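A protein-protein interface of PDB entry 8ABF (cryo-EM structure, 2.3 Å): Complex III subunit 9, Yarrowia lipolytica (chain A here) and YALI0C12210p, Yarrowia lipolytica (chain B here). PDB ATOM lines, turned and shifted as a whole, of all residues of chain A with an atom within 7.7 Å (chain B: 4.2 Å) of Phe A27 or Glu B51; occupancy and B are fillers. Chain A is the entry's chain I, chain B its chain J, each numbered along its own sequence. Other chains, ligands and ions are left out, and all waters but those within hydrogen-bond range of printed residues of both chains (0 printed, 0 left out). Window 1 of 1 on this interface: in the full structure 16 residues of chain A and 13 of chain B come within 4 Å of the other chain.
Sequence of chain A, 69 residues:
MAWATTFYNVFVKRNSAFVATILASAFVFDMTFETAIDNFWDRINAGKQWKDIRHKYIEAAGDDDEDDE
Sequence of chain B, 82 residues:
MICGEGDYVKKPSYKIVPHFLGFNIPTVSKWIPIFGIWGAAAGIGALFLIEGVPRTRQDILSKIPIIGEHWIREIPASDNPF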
ATOM      1  N   THR A  21      -1.422  11.389 -21.947  1.00  0.00           N
ATOM      2  CA  THR A  21      -2.125  12.575 -21.486  1.00  0.00           C
ATOM      3  C   THR A  21      -3.619  12.297 -21.347  1.00  0.00           C
ATOM      4  O   THR A  21      -4.256  12.815 -20.442  1.00  0.00           O
ATOM      5  CB  THR A  21      -1.935  13.712 -22.495  1.00  0.00           C
ATOM      6  OG1 THR A  21      -0.536  13.897 -22.692  1.00  0.00           O
ATOM      7  CG2 THR A  21      -2.558  15.020 -22.062  1.00  0.00           C
ATOM      8  N   ILE A  22      -4.195  11.565 -22.298  1.00  0.00           N
ATOM      9  CA  ILE A  22      -5.610  11.241 -22.244  1.00  0.00           C
ATOM     10  C   ILE A  22      -5.891  10.395 -20.998  1.00  0.00           C
ATOM     11  O   ILE A  22      -6.834  10.702 -20.281  1.00  0.00           O
ATOM     12  CB  ILE A  22      -6.059  10.572 -23.563  1.00  0.00           C
ATOM     13  CG1 ILE A  22      -6.088  11.574 -24.725  1.00  0.00           C
ATOM     14  CG2 ILE A  22      -7.397   9.849 -23.415  1.00  0.00           C
ATOM     15  CD1 ILE A  22      -6.029  10.954 -26.122  1.00  0.00           C
ATOM     16  N   LEU A  23      -5.069   9.359 -20.731  1.00  0.00           N
ATOM     17  CA  LEU A  23      -5.289   8.483 -19.582  1.00  0.00           C
ATOM     18  C   LEU A  23      -5.113   9.229 -18.266  1.00  0.00           C
ATOM     19  O   LEU A  23      -5.917   9.034 -17.365  1.00  0.00           O
ATOM     20  CB  LEU A  23      -4.426   7.218 -19.630  1.00  0.00           C
ATOM     21  CG  LEU A  23      -4.709   6.309 -20.823  1.00  0.00           C
ATOM     22  CD1 LEU A  23      -3.742   5.134 -20.884  1.00  0.00           C
ATOM     23  CD2 LEU A  23      -6.156   5.843 -20.847  1.00  0.00           C
ATOM     24  N   ALA A  24      -4.096  10.092 -18.168  1.00  0.00           N
ATOM     25  CA  ALA A  24      -3.883  10.881 -16.962  1.00  0.00           C
ATOM     26  C   ALA A  24      -5.054  11.839 -16.737  1.00  0.00           C
ATOM     27  O   ALA A  24      -5.511  12.006 -15.610  1.00  0.00           O
ATOM     28  CB  ALA A  24      -2.582  11.626 -17.071  1.00  0.00           C
ATOM     29  N   SER A  25      -5.577  12.422 -17.821  1.00  0.00           N
ATOM     30  CA  SER A  25      -6.725  13.312 -17.724  1.00  0.00           C
ATOM     31  C   SER A  25      -7.966  12.543 -17.296  1.00  0.00           C
ATOM     32  O   SER A  25      -8.802  13.076 -16.572  1.00  0.00           O
ATOM     33  CB  SER A  25      -6.985  13.983 -19.031  1.00  0.00           C
ATOM     34  OG  SER A  25      -5.837  14.706 -19.424  1.00  0.00           O
ATOM     35  N   ALA A  26      -8.102  11.311 -17.791  1.00  0.00           N
ATOM     36  CA  ALA A  26      -9.260  10.510 -17.444  1.00  0.00           C
ATOM     37  C   ALA A  26      -9.233  10.204 -15.947  1.00  0.00           C
ATOM     38  O   ALA A  26     -10.277  10.236 -15.309  1.00  0.00           O
ATOM     39  CB  ALA A  26      -9.303   9.267 -18.295  1.00  0.00           C
ATOM     40  N   PHE A  27      -8.041   9.916 -15.413  1.00  0.00           N
ATOM     41  CA  PHE A  27      -7.840   9.675 -13.992  1.00  0.00           C
ATOM     42  C   PHE A  27      -8.259  10.904 -13.177  1.00  0.00           C
ATOM     43  O   PHE A  27      -9.071  10.793 -12.256  1.00  0.00           O
ATOM     44  CB  PHE A  27      -6.388   9.262 -13.747  1.00  0.00           C
ATOM     45  CG  PHE A  27      -6.134   8.376 -12.554  1.00  0.00           C
ATOM     46  CD1 PHE A  27      -6.855   8.514 -11.373  1.00  0.00           C
ATOM     47  CD2 PHE A  27      -5.131   7.416 -12.600  1.00  0.00           C
ATOM     48  CE1 PHE A  27      -6.600   7.700 -10.276  1.00  0.00           C
ATOM     49  CE2 PHE A  27      -4.869   6.605 -11.501  1.00  0.00           C
ATOM     50  CZ  PHE A  27      -5.605   6.747 -10.342  1.00  0.00           C
ATOM     51  N   VAL A  28      -7.788  12.092 -13.572  1.00  0.00           N
ATOM     52  CA  VAL A  28      -8.160  13.318 -12.880  1.00  0.00           C
ATOM     53  C   VAL A  28      -9.665  13.566 -12.973  1.00  0.00           C
ATOM     54  O   VAL A  28     -10.306  13.836 -11.960  1.00  0.00           O
ATOM     55  CB  VAL A  28      -7.374  14.530 -13.406  1.00  0.00           C
ATOM     56  CG1 VAL A  28      -7.818  15.815 -12.726  1.00  0.00           C
ATOM     57  CG2 VAL A  28      -5.878  14.325 -13.246  1.00  0.00           C
ATOM     58  N   PHE A  29     -10.220  13.465 -14.184  1.00  0.00           N
ATOM     59  CA  PHE A  29     -11.637  13.694 -14.398  1.00  0.00           C
ATOM     60  C   PHE A  29     -12.442  12.800 -13.460  1.00  0.00           C
ATOM     61  O   PHE A  29     -13.290  13.281 -12.714  1.00  0.00           O
ATOM     62  CB  PHE A  29     -12.019  13.470 -15.866  1.00  0.00           C
ATOM     63  CG  PHE A  29     -13.514  13.439 -16.063  1.00  0.00           C
ATOM     64  CD1 PHE A  29     -14.237  14.620 -16.167  1.00  0.00           C
ATOM     65  CD2 PHE A  29     -14.213  12.234 -16.070  1.00  0.00           C
ATOM     66  CE1 PHE A  29     -15.618  14.595 -16.312  1.00  0.00           C
ATOM     67  CE2 PHE A  29     -15.597  12.212 -16.198  1.00  0.00           C
ATOM     68  CZ  PHE A  29     -16.302  13.394 -16.302  1.00  0.00           C
ATOM     69  N   ASP A  30     -12.126  11.505 -13.473  1.00  0.00           N
ATOM     70  CA  ASP A  30     -12.818  10.508 -12.679  1.00  0.00           C
ATOM     71  C   ASP A  30     -12.847  10.881 -11.197  1.00  0.00           C
ATOM     72  O   ASP A  30     -13.887  10.758 -10.564  1.00  0.00           O
ATOM     73  CB  ASP A  30     -12.170   9.137 -12.841  1.00  0.00           C
ATOM     74  CG  ASP A  30     -13.134   7.996 -12.577  1.00  0.00           C
ATOM     75  OD1 ASP A  30     -14.022   7.768 -13.434  1.00  0.00           O
ATOM     76  OD2 ASP A  30     -12.995   7.331 -11.533  1.00  0.00           O
ATOM     77  N   MET A  31     -11.719  11.328 -10.639  1.00  0.00           N
ATOM     78  CA  MET A  31     -11.658  11.654  -9.218  1.00  0.00           C
ATOM     79  C   MET A  31     -12.392  12.957  -8.897  1.00  0.00           C
ATOM     80  O   MET A  31     -13.080  13.055  -7.879  1.00  0.00           O
ATOM     81  CB  MET A  31     -10.207  11.729  -8.744  1.00  0.00           C
ATOM     82  CG  MET A  31      -9.439  10.437  -9.010  1.00  0.00           C
ATOM     83  SD  MET A  31      -9.984   8.918  -8.146  1.00  0.00           S
ATOM     84  CE  MET A  31     -11.000   8.099  -9.380  1.00  0.00           C
ATOM     85  N   THR A  32     -12.263  13.952  -9.770  1.00  0.00           N
ATOM     86  CA  THR A  32     -12.852  15.250  -9.493  1.00  0.00           C
ATOM     87  C   THR A  32     -14.354  15.226  -9.744  1.00  0.00           C
ATOM     88  O   THR A  32     -15.105  15.832  -8.994  1.00  0.00           O
ATOM     89  CB  THR A  32     -12.138  16.353 -10.273  1.00  0.00           C
ATOM     90  OG1 THR A  32     -12.151  15.891 -11.623  1.00  0.00           O
ATOM     91  CG2 THR A  32     -10.699  16.468  -9.835  1.00  0.00           C
ATOM     92  N   PHE A  33     -14.786  14.527 -10.793  1.00  0.00           N
ATOM     93  CA  PHE A  33     -16.197  14.438 -11.117  1.00  0.00           C
ATOM     94  C   PHE A  33     -16.959  13.727 -10.002  1.00  0.00           C
ATOM     95  O   PHE A  33     -18.062  14.137  -9.668  1.00  0.00           O
ATOM     96  CB  PHE A  33     -16.355  13.661 -12.418  1.00  0.00           C
ATOM     97  CG  PHE A  33     -17.748  13.571 -12.973  1.00  0.00           C
ATOM     98  CD1 PHE A  33     -18.468  14.715 -13.293  1.00  0.00           C
ATOM     99  CD2 PHE A  33     -18.289  12.336 -13.295  1.00  0.00           C
ATOM    100  CE1 PHE A  33     -19.727  14.619 -13.870  1.00  0.00           C
ATOM    101  CE2 PHE A  33     -19.536  12.243 -13.895  1.00  0.00           C
ATOM    102  CZ  PHE A  33     -20.261  13.383 -14.168  1.00  0.00           C
ATOM    103  N   GLU A  34     -16.353  12.669  -9.453  1.00  0.00           N
ATOM    104  CA  GLU A  34     -16.894  11.932  -8.323  1.00  0.00           C
ATOM    105  C   GLU A  34     -17.160  12.891  -7.167  1.00  0.00           C
ATOM    106  O   GLU A  34     -18.269  12.944  -6.647  1.00  0.00           O
ATOM    107  CB  GLU A  34     -15.893  10.852  -7.911  1.00  0.00           C
ATOM    108  CG  GLU A  34     -16.374   9.905  -6.827  1.00  0.00           C
ATOM    109  CD  GLU A  34     -15.735  10.048  -5.451  1.00  0.00           C
ATOM    110  OE1 GLU A  34     -15.889   9.113  -4.638  1.00  0.00           O
ATOM    111  OE2 GLU A  34     -15.106  11.096  -5.181  1.00  0.00           O
ATOM    112  N   LEU B  47      -2.911   1.521 -13.289  1.00  0.00           N
ATOM    113  CA  LEU B  47      -3.206   2.021 -11.961  1.00  0.00           C
ATOM    114  C   LEU B  47      -4.627   2.571 -11.901  1.00  0.00           C
ATOM    115  O   LEU B  47      -5.328   2.371 -10.912  1.00  0.00           O
ATOM    116  CB  LEU B  47      -2.188   3.099 -11.601  1.00  0.00           C
ATOM    117  CG  LEU B  47      -2.296   3.640 -10.180  1.00  0.00           C
ATOM    118  CD1 LEU B  47      -2.003   2.541  -9.169  1.00  0.00           C
ATOM    119  CD2 LEU B  47      -1.330   4.797  -9.989  1.00  0.00           C
ATOM    120  N   PHE B  48      -5.017   3.281 -12.958  1.00  0.00           N
ATOM    121  CA  PHE B  48      -6.362   3.798 -13.091  1.00  0.00           C
ATOM    122  C   PHE B  48      -7.386   2.664 -13.070  1.00  0.00           C
ATOM    123  O   PHE B  48      -8.443   2.810 -12.464  1.00  0.00           O
ATOM    124  CB  PHE B  48      -6.452   4.572 -14.402  1.00  0.00           C
ATOM    125  CG  PHE B  48      -7.780   5.234 -14.664  1.00  0.00           C
ATOM    126  CD1 PHE B  48      -8.479   5.881 -13.649  1.00  0.00           C
ATOM    127  CD2 PHE B  48      -8.317   5.238 -15.942  1.00  0.00           C
ATOM    128  CE1 PHE B  48      -9.699   6.497 -13.904  1.00  0.00           C
ATOM    129  CE2 PHE B  48      -9.527   5.869 -16.201  1.00  0.00           C
ATOM    130  CZ  PHE B  48     -10.217   6.497 -15.182  1.00  0.00           C
ATOM    131  N   LEU B  49      -7.078   1.548 -13.745  1.00  0.00           N
ATOM    132  CA  LEU B  49      -8.010   0.426 -13.786  1.00  0.00           C
ATOM    133  C   LEU B  49      -8.233  -0.213 -12.412  1.00  0.00           C
ATOM    134  O   LEU B  49      -9.299  -0.775 -12.160  1.00  0.00           O
ATOM    135  CB  LEU B  49      -7.526  -0.622 -14.784  1.00  0.00           C
ATOM    136  CG  LEU B  49      -7.973  -0.386 -16.221  1.00  0.00           C
ATOM    137  CD1 LEU B  49      -7.329  -1.414 -17.129  1.00  0.00           C
ATOM    138  CD2 LEU B  49      -9.491  -0.435 -16.355  1.00  0.00           C
ATOM    139  N   ILE B  50      -7.225  -0.175 -11.539  1.00  0.00           N
ATOM    140  CA  ILE B  50      -7.374  -0.849 -10.256  1.00  0.00           C
ATOM    141  C   ILE B  50      -7.490   0.164  -9.122  1.00  0.00           C
ATOM    142  O   ILE B  50      -7.281  -0.171  -7.958  1.00  0.00           O
ATOM    143  CB  ILE B  50      -6.228  -1.843 -10.027  1.00  0.00           C
ATOM    144  CG1 ILE B  50      -4.874  -1.129 -10.004  1.00  0.00           C
ATOM    145  CG2 ILE B  50      -6.312  -2.966 -11.051  1.00  0.00           C
ATOM    146  CD1 ILE B  50      -3.785  -1.899  -9.309  1.00  0.00           C
ATOM    147  N   GLU B  51      -7.849   1.397  -9.470  1.00  0.00           N
ATOM    148  CA  GLU B  51      -7.971   2.448  -8.473  1.00  0.00           C
ATOM    149  C   GLU B  51      -9.036   2.079  -7.436  1.00  0.00           C
ATOM    150  O   GLU B  51      -8.958   2.502  -6.290  1.00  0.00           O
ATOM    151  CB  GLU B  51      -8.251   3.769  -9.194  1.00  0.00           C
ATOM    152  CG  GLU B  51      -8.652   4.934  -8.293  1.00  0.00           C
ATOM    153  CD  GLU B  51     -10.077   5.020  -7.753  1.00  0.00           C
ATOM    154  OE1 GLU B  51     -11.017   4.577  -8.459  1.00  0.00           O
ATOM    155  OE2 GLU B  51     -10.259   5.583  -6.633  1.00  0.00           O
ATOM    156  N   GLY B  52     -10.045   1.309  -7.851  1.00  0.00           N
ATOM    157  CA  GLY B  52     -11.128   0.921  -6.959  1.00  0.00           C
ATOM    158  C   GLY B  52     -10.727  -0.177  -5.973  1.00  0.00           C
ATOM    159  O   GLY B  52     -11.292  -0.282  -4.888  1.00  0.00           O
ATOM    160  N   VAL B  53      -9.738  -0.995  -6.330  1.00  0.00           N
ATOM    161  CA  VAL B  53      -9.279  -2.044  -5.436  1.00  0.00           C
ATOM    162  C   VAL B  53      -8.761  -1.428  -4.138  1.00  0.00           C
ATOM    163  O   VAL B  53      -7.926  -0.533  -4.170  1.00  0.00           O
ATOM    164  CB  VAL B  53      -8.198  -2.885  -6.121  1.00  0.00           C
ATOM    165  CG1 VAL B  53      -7.606  -3.923  -5.181  1.00  0.00           C
ATOM    166  CG2 VAL B  53      -8.698  -3.467  -7.434  1.00  0.00           C
ATOM    167  N   ARG B  57      -5.522   1.541  -2.942  1.00  0.00           N
ATOM    168  CA  ARG B  57      -5.732   2.806  -2.261  1.00  0.00           C
ATOM    169  C   ARG B  57      -4.867   2.820  -1.012  1.00  0.00           C
ATOM    170  O   ARG B  57      -4.075   3.746  -0.842  1.00  0.00           O
ATOM    171  CB  ARG B  57      -7.202   3.009  -1.898  1.00  0.00           C
ATOM    172  CG  ARG B  57      -8.151   2.630  -3.021  1.00  0.00           C
ATOM    173  CD  ARG B  57      -9.566   3.001  -2.691  1.00  0.00           C
ATOM    174  NE  ARG B  57     -10.356   3.233  -3.887  1.00  0.00           N
ATOM    175  CZ  ARG B  57     -11.658   3.477  -3.868  1.00  0.00           C
ATOM    176  NH1 ARG B  57     -12.319   3.477  -2.722  1.00  0.00           N
ATOM    177  NH2 ARG B  57     -12.304   3.706  -4.995  1.00  0.00           N
ATOM    178  N   LEU B  61      -2.234   4.782  -3.440  1.00  0.00           N
ATOM    179  CA  LEU B  61      -2.837   6.070  -3.744  1.00  0.00           C
ATOM    180  C   LEU B  61      -2.926   6.973  -2.514  1.00  0.00           C
ATOM    181  O   LEU B  61      -2.847   8.187  -2.651  1.00  0.00           O
ATOM    182  CB  LEU B  61      -4.208   5.862  -4.392  1.00  0.00           C
ATOM    183  CG  LEU B  61      -4.198   5.209  -5.777  1.00  0.00           C
ATOM    184  CD1 LEU B  61      -5.612   4.909  -6.260  1.00  0.00           C
ATOM    185  CD2 LEU B  61      -3.470   6.074  -6.799  1.00  0.00           C
ATOM    186  N   TRP B  71      -8.275   9.370  -0.856  1.00  0.00           N
ATOM    187  CA  TRP B  71      -8.516   7.938  -0.755  1.00  0.00           C
ATOM    188  C   TRP B  71      -8.551   7.455   0.692  1.00  0.00           C
ATOM    189  O   TRP B  71      -8.648   6.253   0.935  1.00  0.00           O
ATOM    190  CB  TRP B  71      -7.502   7.144  -1.584  1.00  0.00           C
ATOM    191  CG  TRP B  71      -7.655   7.354  -3.057  1.00  0.00           C
ATOM    192  CD1 TRP B  71      -8.543   6.739  -3.888  1.00  0.00           C
ATOM    193  CD2 TRP B  71      -6.896   8.247  -3.886  1.00  0.00           C
ATOM    194  NE1 TRP B  71      -8.381   7.169  -5.175  1.00  0.00           N
ATOM    195  CE2 TRP B  71      -7.387   8.103  -5.206  1.00  0.00           C
ATOM    196  CE3 TRP B  71      -5.845   9.138  -3.644  1.00  0.00           C
ATOM    197  CZ2 TRP B  71      -6.855   8.810  -6.281  1.00  0.00           C
ATOM    198  CZ3 TRP B  71      -5.328   9.849  -4.705  1.00  0.00           C
ATOM    199  CH2 TRP B  71      -5.829   9.683  -6.001  1.00  0.00           C
ATOM    200  N   ARG B  73     -10.930   7.390   3.372  1.00  0.00           N
ATOM    201  CA  ARG B  73     -12.335   7.585   3.694  1.00  0.00           C
ATOM    202  C   ARG B  73     -12.801   6.466   4.620  1.00  0.00           C
ATOM    203  O   ARG B  73     -12.641   5.291   4.294  1.00  0.00           O
ATOM    204  CB  ARG B  73     -13.189   7.710   2.425  1.00  0.00           C
ATOM    205  CG  ARG B  73     -12.615   7.016   1.199  1.00  0.00           C
ATOM    206  CD  ARG B  73     -13.621   6.850   0.079  1.00  0.00           C
ATOM    207  NE  ARG B  73     -12.987   6.591  -1.208  1.00  0.00           N
ATOM    208  CZ  ARG B  73     -12.899   7.467  -2.206  1.00  0.00           C
ATOM    209  NH1 ARG B  73     -13.413   8.680  -2.081  1.00  0.00           N
ATOM    210  NH2 ARG B  73     -12.304   7.128  -3.336  1.00  0.00           N
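The guanidinium group of Arg B73 lies within salt-bridge range of the side-chain carboxylate of Glu A34, at 3.6 Å. SD of Met A31 lies close to OE2 of Glu B51 (3.7 Å).
OE2 of Glu B51 is in salt-bridge range of NH2 of Arg B57, 3.2 Å away. The side-chain carboxylate (OE2) of Glu B51 lies within hydrogen-bond range of the indole nitrogen (NE1) of Trp B71.
Among the printed residues, pairs that only touch across the chains: Phe A27 with Phe B48 (3.6 Å), Met A31 with Trp B71 (3.6 Å), Ala A26 with Phe B48 (3.7 Å), Asp A30 with Phe B48 (3.8 Å) and Phe A27 with Glu B51 (3.97 Å).
Of the printed residues of chain B, Phe A27 touches Phe B48 and Glu B51. Of the printed residues of chain A, Glu B51 touches Phe A27 (3.97 Å) and Met A31 (3.6 Å). Of the printed residues of chain B, Met A31 touches Glu B51 and Trp B71. Printed residues of chain A within 4 Å of Phe B48: Ala A26, Phe A27 and Asp A30. Of the printed residues of chain A, Trp B71 touches Met A31. Printed residues of chain B within 4 Å of Asp A30: Phe B48 (3.8 Å). Printed residues of chain B within 4 Å of Glu A34: Arg B73 (3.6 Å). The nearest residue of chain B that does not touch Phe A27 is Leu B47 (4.1 Å). The nearest residue of chain A that does not touch Glu B51 is Asp A30 (4.6 Å). The nearest printed residue of chain A that does not touch Phe B48 is Leu A23 (4.7 Å).
Of the 11 printed residues of chain B, 4 touch a printed residue of chain A. Printed residues of chain B that touch a printed residue of chain A: Phe B48, Glu B51, Trp B71 and Arg B73. Hydrophobic or aromatic side chains of chain B that line the printed part of chain A: Phe B48 and Trp B71. Of the 14 printed residues of chain A, 5 touch a printed residue of chain B. Printed residues of chain A that touch a printed residue of chain B: Ala A26, Phe A27, Asp A30, Met A31 and Glu A34. Hydrophobic or aromatic side chains of chain A within 4 Å of the printed part of chain B: Ala A26, Phe A27 and Met A31. Along chain A the printed residues that touch a printed residue of chain B span positions 26 to 34. Among the printed residues, 7 pairs touch across the chains. Among the printed residues, Asp or Glu carboxylates within 4 Å of a Lys or Arg side-chain nitrogen of the other chain: Glu A34 with Arg B73 (3.6 Å).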
